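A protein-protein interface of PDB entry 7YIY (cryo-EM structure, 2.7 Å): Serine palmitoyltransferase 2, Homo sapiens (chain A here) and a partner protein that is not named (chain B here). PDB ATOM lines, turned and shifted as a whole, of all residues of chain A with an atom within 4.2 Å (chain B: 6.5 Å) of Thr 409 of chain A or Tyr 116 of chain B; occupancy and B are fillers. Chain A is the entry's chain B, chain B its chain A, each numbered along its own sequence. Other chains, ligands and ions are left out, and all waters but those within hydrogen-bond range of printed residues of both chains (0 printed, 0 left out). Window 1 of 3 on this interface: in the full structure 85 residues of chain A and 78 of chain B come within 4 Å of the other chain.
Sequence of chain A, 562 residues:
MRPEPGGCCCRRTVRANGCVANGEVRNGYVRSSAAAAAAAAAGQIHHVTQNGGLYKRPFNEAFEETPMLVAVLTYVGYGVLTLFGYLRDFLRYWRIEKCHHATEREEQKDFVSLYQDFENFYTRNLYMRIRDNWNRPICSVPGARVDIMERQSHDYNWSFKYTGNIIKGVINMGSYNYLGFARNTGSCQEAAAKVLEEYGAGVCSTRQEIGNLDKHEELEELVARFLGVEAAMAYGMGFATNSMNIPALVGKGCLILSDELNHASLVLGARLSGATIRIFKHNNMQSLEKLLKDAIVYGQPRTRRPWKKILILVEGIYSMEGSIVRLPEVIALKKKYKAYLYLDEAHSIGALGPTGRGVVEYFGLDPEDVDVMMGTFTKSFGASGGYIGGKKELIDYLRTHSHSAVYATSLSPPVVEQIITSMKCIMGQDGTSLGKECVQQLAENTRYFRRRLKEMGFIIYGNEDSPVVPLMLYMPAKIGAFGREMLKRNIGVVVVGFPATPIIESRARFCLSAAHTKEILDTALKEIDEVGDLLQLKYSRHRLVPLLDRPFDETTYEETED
The side-chain sulfur (SD) of Met 237 of chain A sits at hydrogen-bond distance from the backbone NH (N) of Ala 240 of chain A, at 3.7 Å. The side-chain amide nitrogen (ND2) of Asn 256 of chain B sits at hydrogen-bond distance from the side-chain carboxylate (OE2) of Glu 258 of chain B, at 2.9 Å.
Printed residues of chain B that touch a printed residue of chain A: Tyr 116 and Glu 258. Of the 10 printed residues of chain A, 7 touch a printed residue of chain B. Printed residues of chain A that touch a printed residue of chain B: Tyr 235, Gly 236, Met 237, Ala 240, Ser 404, Ala 408 and Thr 409. Hydrophobic or aromatic side chains of chain A that line the printed part of chain B: Met 237, Ala 240 and Ala 408. Among the printed residues, 8 pairs touch across the chains. Among the printed residues, no Asp or Glu carboxylate lies within 4 Å of a Lys or Arg side-chain nitrogen of the other chain.
Thr 409 of chain A touches just these residues of chain B: Tyr 116 and Glu 258. Of the printed residues of chain A, Tyr 116 of chain B touches Tyr 235, Gly 236, Met 237, Ala 240, Ser 404, Ala 408 and Thr 409. Of the printed residues of chain B, Tyr 235 of chain A touches Tyr 116 (3.995 Å). Of the printed residues of chain B, Gly 236 of chain A touches Tyr 116. Of the printed residues of chain B, Ser 404 of chain A touches Tyr 116 (3.8 Å). The nearest printed residue of chain B that does not touch Tyr 235 of chain A is Ile 264 of chain B (8.5 Å).
Among the printed residues, merely in contact across the chains: Tyr 235 of chain A with Tyr 116 of chain B (3.995 Å), Gly 236 of chain A with Tyr 116 of chain B (3.99 Å), Met 237 of chain A with Tyr 116 of chain B (3.5 Å), Ala 240 of chain A with Tyr 116 of chain B (3.8 Å), Ser 404 of chain A with Tyr 116 of chain B (3.8 Å), Ala 408 of chain A with Tyr 116 of chain B (3.1 Å) and Thr 409 of chain A with Tyr 116 of chain B (3.9 Å).
The side-chain hydroxyl of Thr 409 of chain A sits at hydrogen-bond distance from the side-chain carboxylate of Glu 258 of chain B (3.3 Å).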
ATOM      1  N   VAL A 203      11.373  31.085 -13.260  1.00  0.00           N
ATOM      2  CA  VAL A 203      12.345  31.611 -12.312  1.00  0.00           C
ATOM      3  C   VAL A 203      12.879  30.379 -11.596  1.00  0.00           C
ATOM      4  O   VAL A 203      12.174  29.369 -11.491  1.00  0.00           O
ATOM      5  CB  VAL A 203      11.696  32.615 -11.342  1.00  0.00           C
ATOM      6  CG1 VAL A 203      12.686  33.105 -10.311  1.00  0.00           C
ATOM      7  CG2 VAL A 203      11.101  33.773 -12.095  1.00  0.00           C
ATOM      8  N   SER A 205      14.366  30.321  -8.308  1.00  0.00           N
ATOM      9  CA  SER A 205      14.738  30.666  -6.944  1.00  0.00           C
ATOM     10  C   SER A 205      13.572  31.386  -6.278  1.00  0.00           C
ATOM     11  O   SER A 205      12.490  31.523  -6.855  1.00  0.00           O
ATOM     12  CB  SER A 205      16.008  31.517  -6.921  1.00  0.00           C
ATOM     13  OG  SER A 205      16.418  31.798  -5.597  1.00  0.00           O
ATOM     14  N   TYR A 235       2.270  36.989  -5.180  1.00  0.00           N
ATOM     15  CA  TYR A 235       2.618  35.661  -4.679  1.00  0.00           C
ATOM     16  C   TYR A 235       2.829  34.598  -5.748  1.00  0.00           C
ATOM     17  O   TYR A 235       3.894  33.977  -5.767  1.00  0.00           O
ATOM     18  CB  TYR A 235       1.568  35.224  -3.660  1.00  0.00           C
ATOM     19  CG  TYR A 235       1.738  36.023  -2.410  1.00  0.00           C
ATOM     20  CD1 TYR A 235       2.787  35.761  -1.550  1.00  0.00           C
ATOM     21  CD2 TYR A 235       0.898  37.076  -2.115  1.00  0.00           C
ATOM     22  CE1 TYR A 235       2.978  36.501  -0.430  1.00  0.00           C
ATOM     23  CE2 TYR A 235       1.081  37.818  -0.990  1.00  0.00           C
ATOM     24  CZ  TYR A 235       2.123  37.526  -0.149  1.00  0.00           C
ATOM     25  OH  TYR A 235       2.309  38.263   0.989  1.00  0.00           O
ATOM     26  N   GLY A 236       1.876  34.337  -6.625  1.00  0.00           N
ATOM     27  CA  GLY A 236       2.116  33.241  -7.546  1.00  0.00           C
ATOM     28  C   GLY A 236       1.050  32.172  -7.613  1.00  0.00           C
ATOM     29  O   GLY A 236       1.014  31.390  -8.562  1.00  0.00           O
ATOM     30  N   MET A 237       0.177  32.128  -6.614  1.00  0.00           N
ATOM     31  CA  MET A 237      -0.976  31.243  -6.617  1.00  0.00           C
ATOM     32  C   MET A 237      -2.018  31.853  -5.699  1.00  0.00           C
ATOM     33  O   MET A 237      -1.661  32.469  -4.694  1.00  0.00           O
ATOM     34  CB  MET A 237      -0.589  29.837  -6.155  1.00  0.00           C
ATOM     35  CG  MET A 237      -1.708  28.824  -6.132  1.00  0.00           C
ATOM     36  SD  MET A 237      -1.229  27.407  -5.140  1.00  0.00           S
ATOM     37  CE  MET A 237      -2.541  26.263  -5.469  1.00  0.00           C
ATOM     38  N   ALA A 240      -2.524  29.604  -2.403  1.00  0.00           N
ATOM     39  CA  ALA A 240      -1.363  29.835  -1.564  1.00  0.00           C
ATOM     40  C   ALA A 240      -1.376  31.195  -0.888  1.00  0.00           C
ATOM     41  O   ALA A 240      -0.927  31.293   0.253  1.00  0.00           O
ATOM     42  CB  ALA A 240      -0.093  29.688  -2.395  1.00  0.00           C
ATOM     43  N   SER A 404       5.585  31.823   1.671  1.00  0.00           N
ATOM     44  CA  SER A 404       5.815  31.914   0.235  1.00  0.00           C
ATOM     45  C   SER A 404       7.106  32.652  -0.084  1.00  0.00           C
ATOM     46  O   SER A 404       7.883  32.208  -0.934  1.00  0.00           O
ATOM     47  CB  SER A 404       4.637  32.608  -0.441  1.00  0.00           C
ATOM     48  OG  SER A 404       3.540  31.737  -0.594  1.00  0.00           O
ATOM     49  N   ALA A 408       9.008  29.370  -1.563  1.00  0.00           N
ATOM     50  CA  ALA A 408       8.338  29.113  -2.828  1.00  0.00           C
ATOM     51  C   ALA A 408       8.935  29.947  -3.957  1.00  0.00           C
ATOM     52  O   ALA A 408       9.503  31.017  -3.741  1.00  0.00           O
ATOM     53  CB  ALA A 408       6.844  29.390  -2.700  1.00  0.00           C
ATOM     54  N   THR A 409       8.789  29.440  -5.179  1.00  0.00           N
ATOM     55  CA  THR A 409       9.271  30.115  -6.378  1.00  0.00           C
ATOM     56  C   THR A 409       8.367  31.291  -6.725  1.00  0.00           C
ATOM     57  O   THR A 409       7.160  31.252  -6.483  1.00  0.00           O
ATOM     58  CB  THR A 409       9.338  29.134  -7.551  1.00  0.00           C
ATOM     59  OG1 THR A 409      10.136  28.008  -7.179  1.00  0.00           O
ATOM     60  CG2 THR A 409       9.967  29.773  -8.778  1.00  0.00           C
ATOM     61  N   SER A 410       8.958  32.335  -7.297  1.00  0.00           N
ATOM     62  CA  SER A 410       8.232  33.561  -7.576  1.00  0.00           C
ATOM     63  C   SER A 410       7.526  33.495  -8.935  1.00  0.00           C
ATOM     64  O   SER A 410       7.668  32.535  -9.692  1.00  0.00           O
ATOM     65  CB  SER A 410       9.184  34.749  -7.500  1.00  0.00           C
ATOM     66  OG  SER A 410      10.268  34.593  -8.387  1.00  0.00           O
ATOM     67  N   TYR B 114       0.235  19.697 -10.528  1.00  0.00           N
ATOM     68  CA  TYR B 114      -0.241  20.842  -9.769  1.00  0.00           C
ATOM     69  C   TYR B 114       0.305  22.116 -10.396  1.00  0.00           C
ATOM     70  O   TYR B 114       1.295  22.099 -11.130  1.00  0.00           O
ATOM     71  CB  TYR B 114       0.195  20.743  -8.305  1.00  0.00           C
ATOM     72  CG  TYR B 114      -0.533  19.699  -7.499  1.00  0.00           C
ATOM     73  CD1 TYR B 114      -1.491  20.065  -6.577  1.00  0.00           C
ATOM     74  CD2 TYR B 114      -0.247  18.353  -7.643  1.00  0.00           C
ATOM     75  CE1 TYR B 114      -2.155  19.135  -5.841  1.00  0.00           C
ATOM     76  CE2 TYR B 114      -0.909  17.411  -6.905  1.00  0.00           C
ATOM     77  CZ  TYR B 114      -1.864  17.811  -6.004  1.00  0.00           C
ATOM     78  OH  TYR B 114      -2.537  16.886  -5.250  1.00  0.00           O
ATOM     79  N   SER B 115      -0.347  23.235 -10.109  1.00  0.00           N
ATOM     80  CA  SER B 115       0.051  24.505 -10.696  1.00  0.00           C
ATOM     81  C   SER B 115       1.080  25.242  -9.855  1.00  0.00           C
ATOM     82  O   SER B 115       1.568  26.293 -10.272  1.00  0.00           O
ATOM     83  CB  SER B 115      -1.172  25.389 -10.934  1.00  0.00           C
ATOM     84  OG  SER B 115      -1.834  25.693  -9.728  1.00  0.00           O
ATOM     85  N   TYR B 116       1.451  24.698  -8.703  1.00  0.00           N
ATOM     86  CA  TYR B 116       2.379  25.374  -7.813  1.00  0.00           C
ATOM     87  C   TYR B 116       3.253  24.321  -7.156  1.00  0.00           C
ATOM     88  O   TYR B 116       2.738  23.328  -6.642  1.00  0.00           O
ATOM     89  CB  TYR B 116       1.594  26.187  -6.790  1.00  0.00           C
ATOM     90  CG  TYR B 116       2.346  27.261  -6.066  1.00  0.00           C
ATOM     91  CD1 TYR B 116       2.848  28.347  -6.755  1.00  0.00           C
ATOM     92  CD2 TYR B 116       2.429  27.271  -4.685  1.00  0.00           C
ATOM     93  CE1 TYR B 116       3.502  29.352  -6.110  1.00  0.00           C
ATOM     94  CE2 TYR B 116       3.073  28.286  -4.025  1.00  0.00           C
ATOM     95  CZ  TYR B 116       3.601  29.329  -4.748  1.00  0.00           C
ATOM     96  OH  TYR B 116       4.243  30.356  -4.115  1.00  0.00           O
ATOM     97  N   GLY B 117       4.568  24.527  -7.192  1.00  0.00           N
ATOM     98  CA  GLY B 117       5.486  23.497  -6.739  1.00  0.00           C
ATOM     99  C   GLY B 117       5.412  23.214  -5.255  1.00  0.00           C
ATOM    100  O   GLY B 117       5.679  22.092  -4.822  1.00  0.00           O
ATOM    101  N   PHE B 118       5.072  24.219  -4.455  1.00  0.00           N
ATOM    102  CA  PHE B 118       4.994  24.050  -3.013  1.00  0.00           C
ATOM    103  C   PHE B 118       3.744  23.300  -2.577  1.00  0.00           C
ATOM    104  O   PHE B 118       3.776  22.616  -1.551  1.00  0.00           O
ATOM    105  CB  PHE B 118       5.045  25.422  -2.334  1.00  0.00           C
ATOM    106  CG  PHE B 118       5.391  25.371  -0.876  1.00  0.00           C
ATOM    107  CD1 PHE B 118       6.694  25.541  -0.458  1.00  0.00           C
ATOM    108  CD2 PHE B 118       4.411  25.162   0.077  1.00  0.00           C
ATOM    109  CE1 PHE B 118       7.015  25.494   0.875  1.00  0.00           C
ATOM    110  CE2 PHE B 118       4.727  25.113   1.415  1.00  0.00           C
ATOM    111  CZ  PHE B 118       6.028  25.284   1.814  1.00  0.00           C
ATOM    112  N   ALA B 119       2.656  23.401  -3.331  1.00  0.00           N
ATOM    113  CA  ALA B 119       1.391  22.785  -2.967  1.00  0.00           C
ATOM    114  C   ALA B 119       1.319  21.302  -3.296  1.00  0.00           C
ATOM    115  O   ALA B 119       0.484  20.605  -2.721  1.00  0.00           O
ATOM    116  CB  ALA B 119       0.238  23.517  -3.654  1.00  0.00           C
ATOM    117  N   THR B 120       2.189  20.791  -4.168  1.00  0.00           N
ATOM    118  CA  THR B 120       2.031  19.414  -4.621  1.00  0.00           C
ATOM    119  C   THR B 120       2.222  18.417  -3.481  1.00  0.00           C
ATOM    120  O   THR B 120       1.403  17.509  -3.317  1.00  0.00           O
ATOM    121  CB  THR B 120       2.972  19.120  -5.799  1.00  0.00           C
ATOM    122  OG1 THR B 120       2.748  17.791  -6.279  1.00  0.00           O
ATOM    123  CG2 THR B 120       4.413  19.268  -5.426  1.00  0.00           C
ATOM    124  N   ILE B 121       3.258  18.584  -2.661  1.00  0.00           N
ATOM    125  CA  ILE B 121       3.475  17.679  -1.538  1.00  0.00           C
ATOM    126  C   ILE B 121       2.727  18.120  -0.284  1.00  0.00           C
ATOM    127  O   ILE B 121       2.385  17.269   0.548  1.00  0.00           O
ATOM    128  CB  ILE B 121       4.983  17.502  -1.249  1.00  0.00           C
ATOM    129  CG1 ILE B 121       5.222  16.348  -0.277  1.00  0.00           C
ATOM    130  CG2 ILE B 121       5.587  18.755  -0.692  1.00  0.00           C
ATOM    131  CD1 ILE B 121       4.869  14.991  -0.830  1.00  0.00           C
ATOM    132  N   ASN B 256       9.037  18.719  -8.275  1.00  0.00           N
ATOM    133  CA  ASN B 256       8.547  19.977  -8.806  1.00  0.00           C
ATOM    134  C   ASN B 256       9.222  20.266 -10.137  1.00  0.00           C
ATOM    135  O   ASN B 256      10.337  19.813 -10.401  1.00  0.00           O
ATOM    136  CB  ASN B 256       8.740  21.139  -7.811  1.00  0.00           C
ATOM    137  CG  ASN B 256      10.184  21.549  -7.628  1.00  0.00           C
ATOM    138  OD1 ASN B 256      11.110  20.881  -8.074  1.00  0.00           O
ATOM    139  ND2 ASN B 256      10.381  22.666  -6.954  1.00  0.00           N
ATOM    140  N   GLU B 258      10.377  22.985 -11.411  1.00  0.00           N
ATOM    141  CA  GLU B 258      10.978  24.304 -11.348  1.00  0.00           C
ATOM    142  C   GLU B 258      12.493  24.301 -11.207  1.00  0.00           C
ATOM    143  O   GLU B 258      13.101  25.367 -11.322  1.00  0.00           O
ATOM    144  CB  GLU B 258      10.363  25.100 -10.195  1.00  0.00           C
ATOM    145  CG  GLU B 258       8.858  25.004 -10.141  1.00  0.00           C
ATOM    146  CD  GLU B 258       8.293  25.421  -8.811  1.00  0.00           C
ATOM    147  OE1 GLU B 258       7.277  26.145  -8.796  1.00  0.00           O
ATOM    148  OE2 GLU B 258       8.873  25.037  -7.776  1.00  0.00           O
ATOM    149  N   ASN B 259      13.126  23.152 -10.978  1.00  0.00           N
ATOM    150  CA  ASN B 259      14.570  23.108 -10.796  1.00  0.00           C
ATOM    151  C   ASN B 259      15.298  22.709 -12.072  1.00  0.00           C
ATOM    152  O   ASN B 259      16.024  23.519 -12.644  1.00  0.00           O
ATOM    153  CB  ASN B 259      14.925  22.141  -9.662  1.00  0.00           C
ATOM    154  CG  ASN B 259      14.568  22.681  -8.300  1.00  0.00           C
ATOM    155  OD1 ASN B 259      14.233  23.847  -8.151  1.00  0.00           O
ATOM    156  ND2 ASN B 259      14.657  21.833  -7.293  1.00  0.00           N
ATOM    157  N   SER B 263      10.633  25.608 -15.034  1.00  0.00           N
ATOM    158  CA  SER B 263       9.249  25.938 -15.322  1.00  0.00           C
ATOM    159  C   SER B 263       8.559  26.174 -13.986  1.00  0.00           C
ATOM    160  O   SER B 263       9.217  26.465 -12.984  1.00  0.00           O
ATOM    161  CB  SER B 263       8.611  24.829 -16.174  1.00  0.00           C
ATOM    162  OG  SER B 263       7.366  25.236 -16.691  1.00  0.00           O
ATOM    163  N   ILE B 264       7.233  26.082 -13.967  1.00  0.00           N
ATOM    164  CA  ILE B 264       6.440  26.265 -12.759  1.00  0.00           C
ATOM    165  C   ILE B 264       5.593  25.018 -12.552  1.00  0.00           C
ATOM    166  O   ILE B 264       5.212  24.357 -13.521  1.00  0.00           O
ATOM    167  CB  ILE B 264       5.549  27.525 -12.860  1.00  0.00           C
ATOM    168  CG1 ILE B 264       6.355  28.726 -13.357  1.00  0.00           C
ATOM    169  CG2 ILE B 264       4.935  27.869 -11.528  1.00  0.00           C
ATOM    170  CD1 ILE B 264       7.424  29.208 -12.408  1.00  0.00           C
ATOM    171  N   GLY B 265       5.313  24.687 -11.300  1.00  0.00           N
ATOM    172  CA  GLY B 265       4.392  23.623 -10.959  1.00  0.00           C
ATOM    173  C   GLY B 265       5.093  22.416 -10.367  1.00  0.00           C
ATOM    174  O   GLY B 265       6.311  22.376 -10.216  1.00  0.00           O
ATOM    175  N   GLY B 266       4.283  21.407 -10.043  1.00  0.00           N
ATOM    176  CA  GLY B 266       4.793  20.153  -9.536  1.00  0.00           C
ATOM    177  C   GLY B 266       3.966  18.992 -10.050  1.00  0.00           C
ATOM    178  O   GLY B 266       2.959  19.182 -10.724  1.00  0.00           O
ATOM    179  N   LEU B 291      -2.717  25.021 -14.424  1.00  0.00           N
ATOM    180  CA  LEU B 291      -1.452  25.585 -14.891  1.00  0.00           C
ATOM    181  C   LEU B 291      -1.621  26.254 -16.251  1.00  0.00           C
ATOM    182  O   LEU B 291      -2.205  25.657 -17.155  1.00  0.00           O
ATOM    183  CB  LEU B 291      -0.401  24.487 -14.992  1.00  0.00           C
ATOM    184  CG  LEU B 291       1.027  24.856 -15.382  1.00  0.00           C
ATOM    185  CD1 LEU B 291       1.753  25.480 -14.216  1.00  0.00           C
ATOM    186  CD2 LEU B 291       1.767  23.643 -15.894  1.00  0.00           C
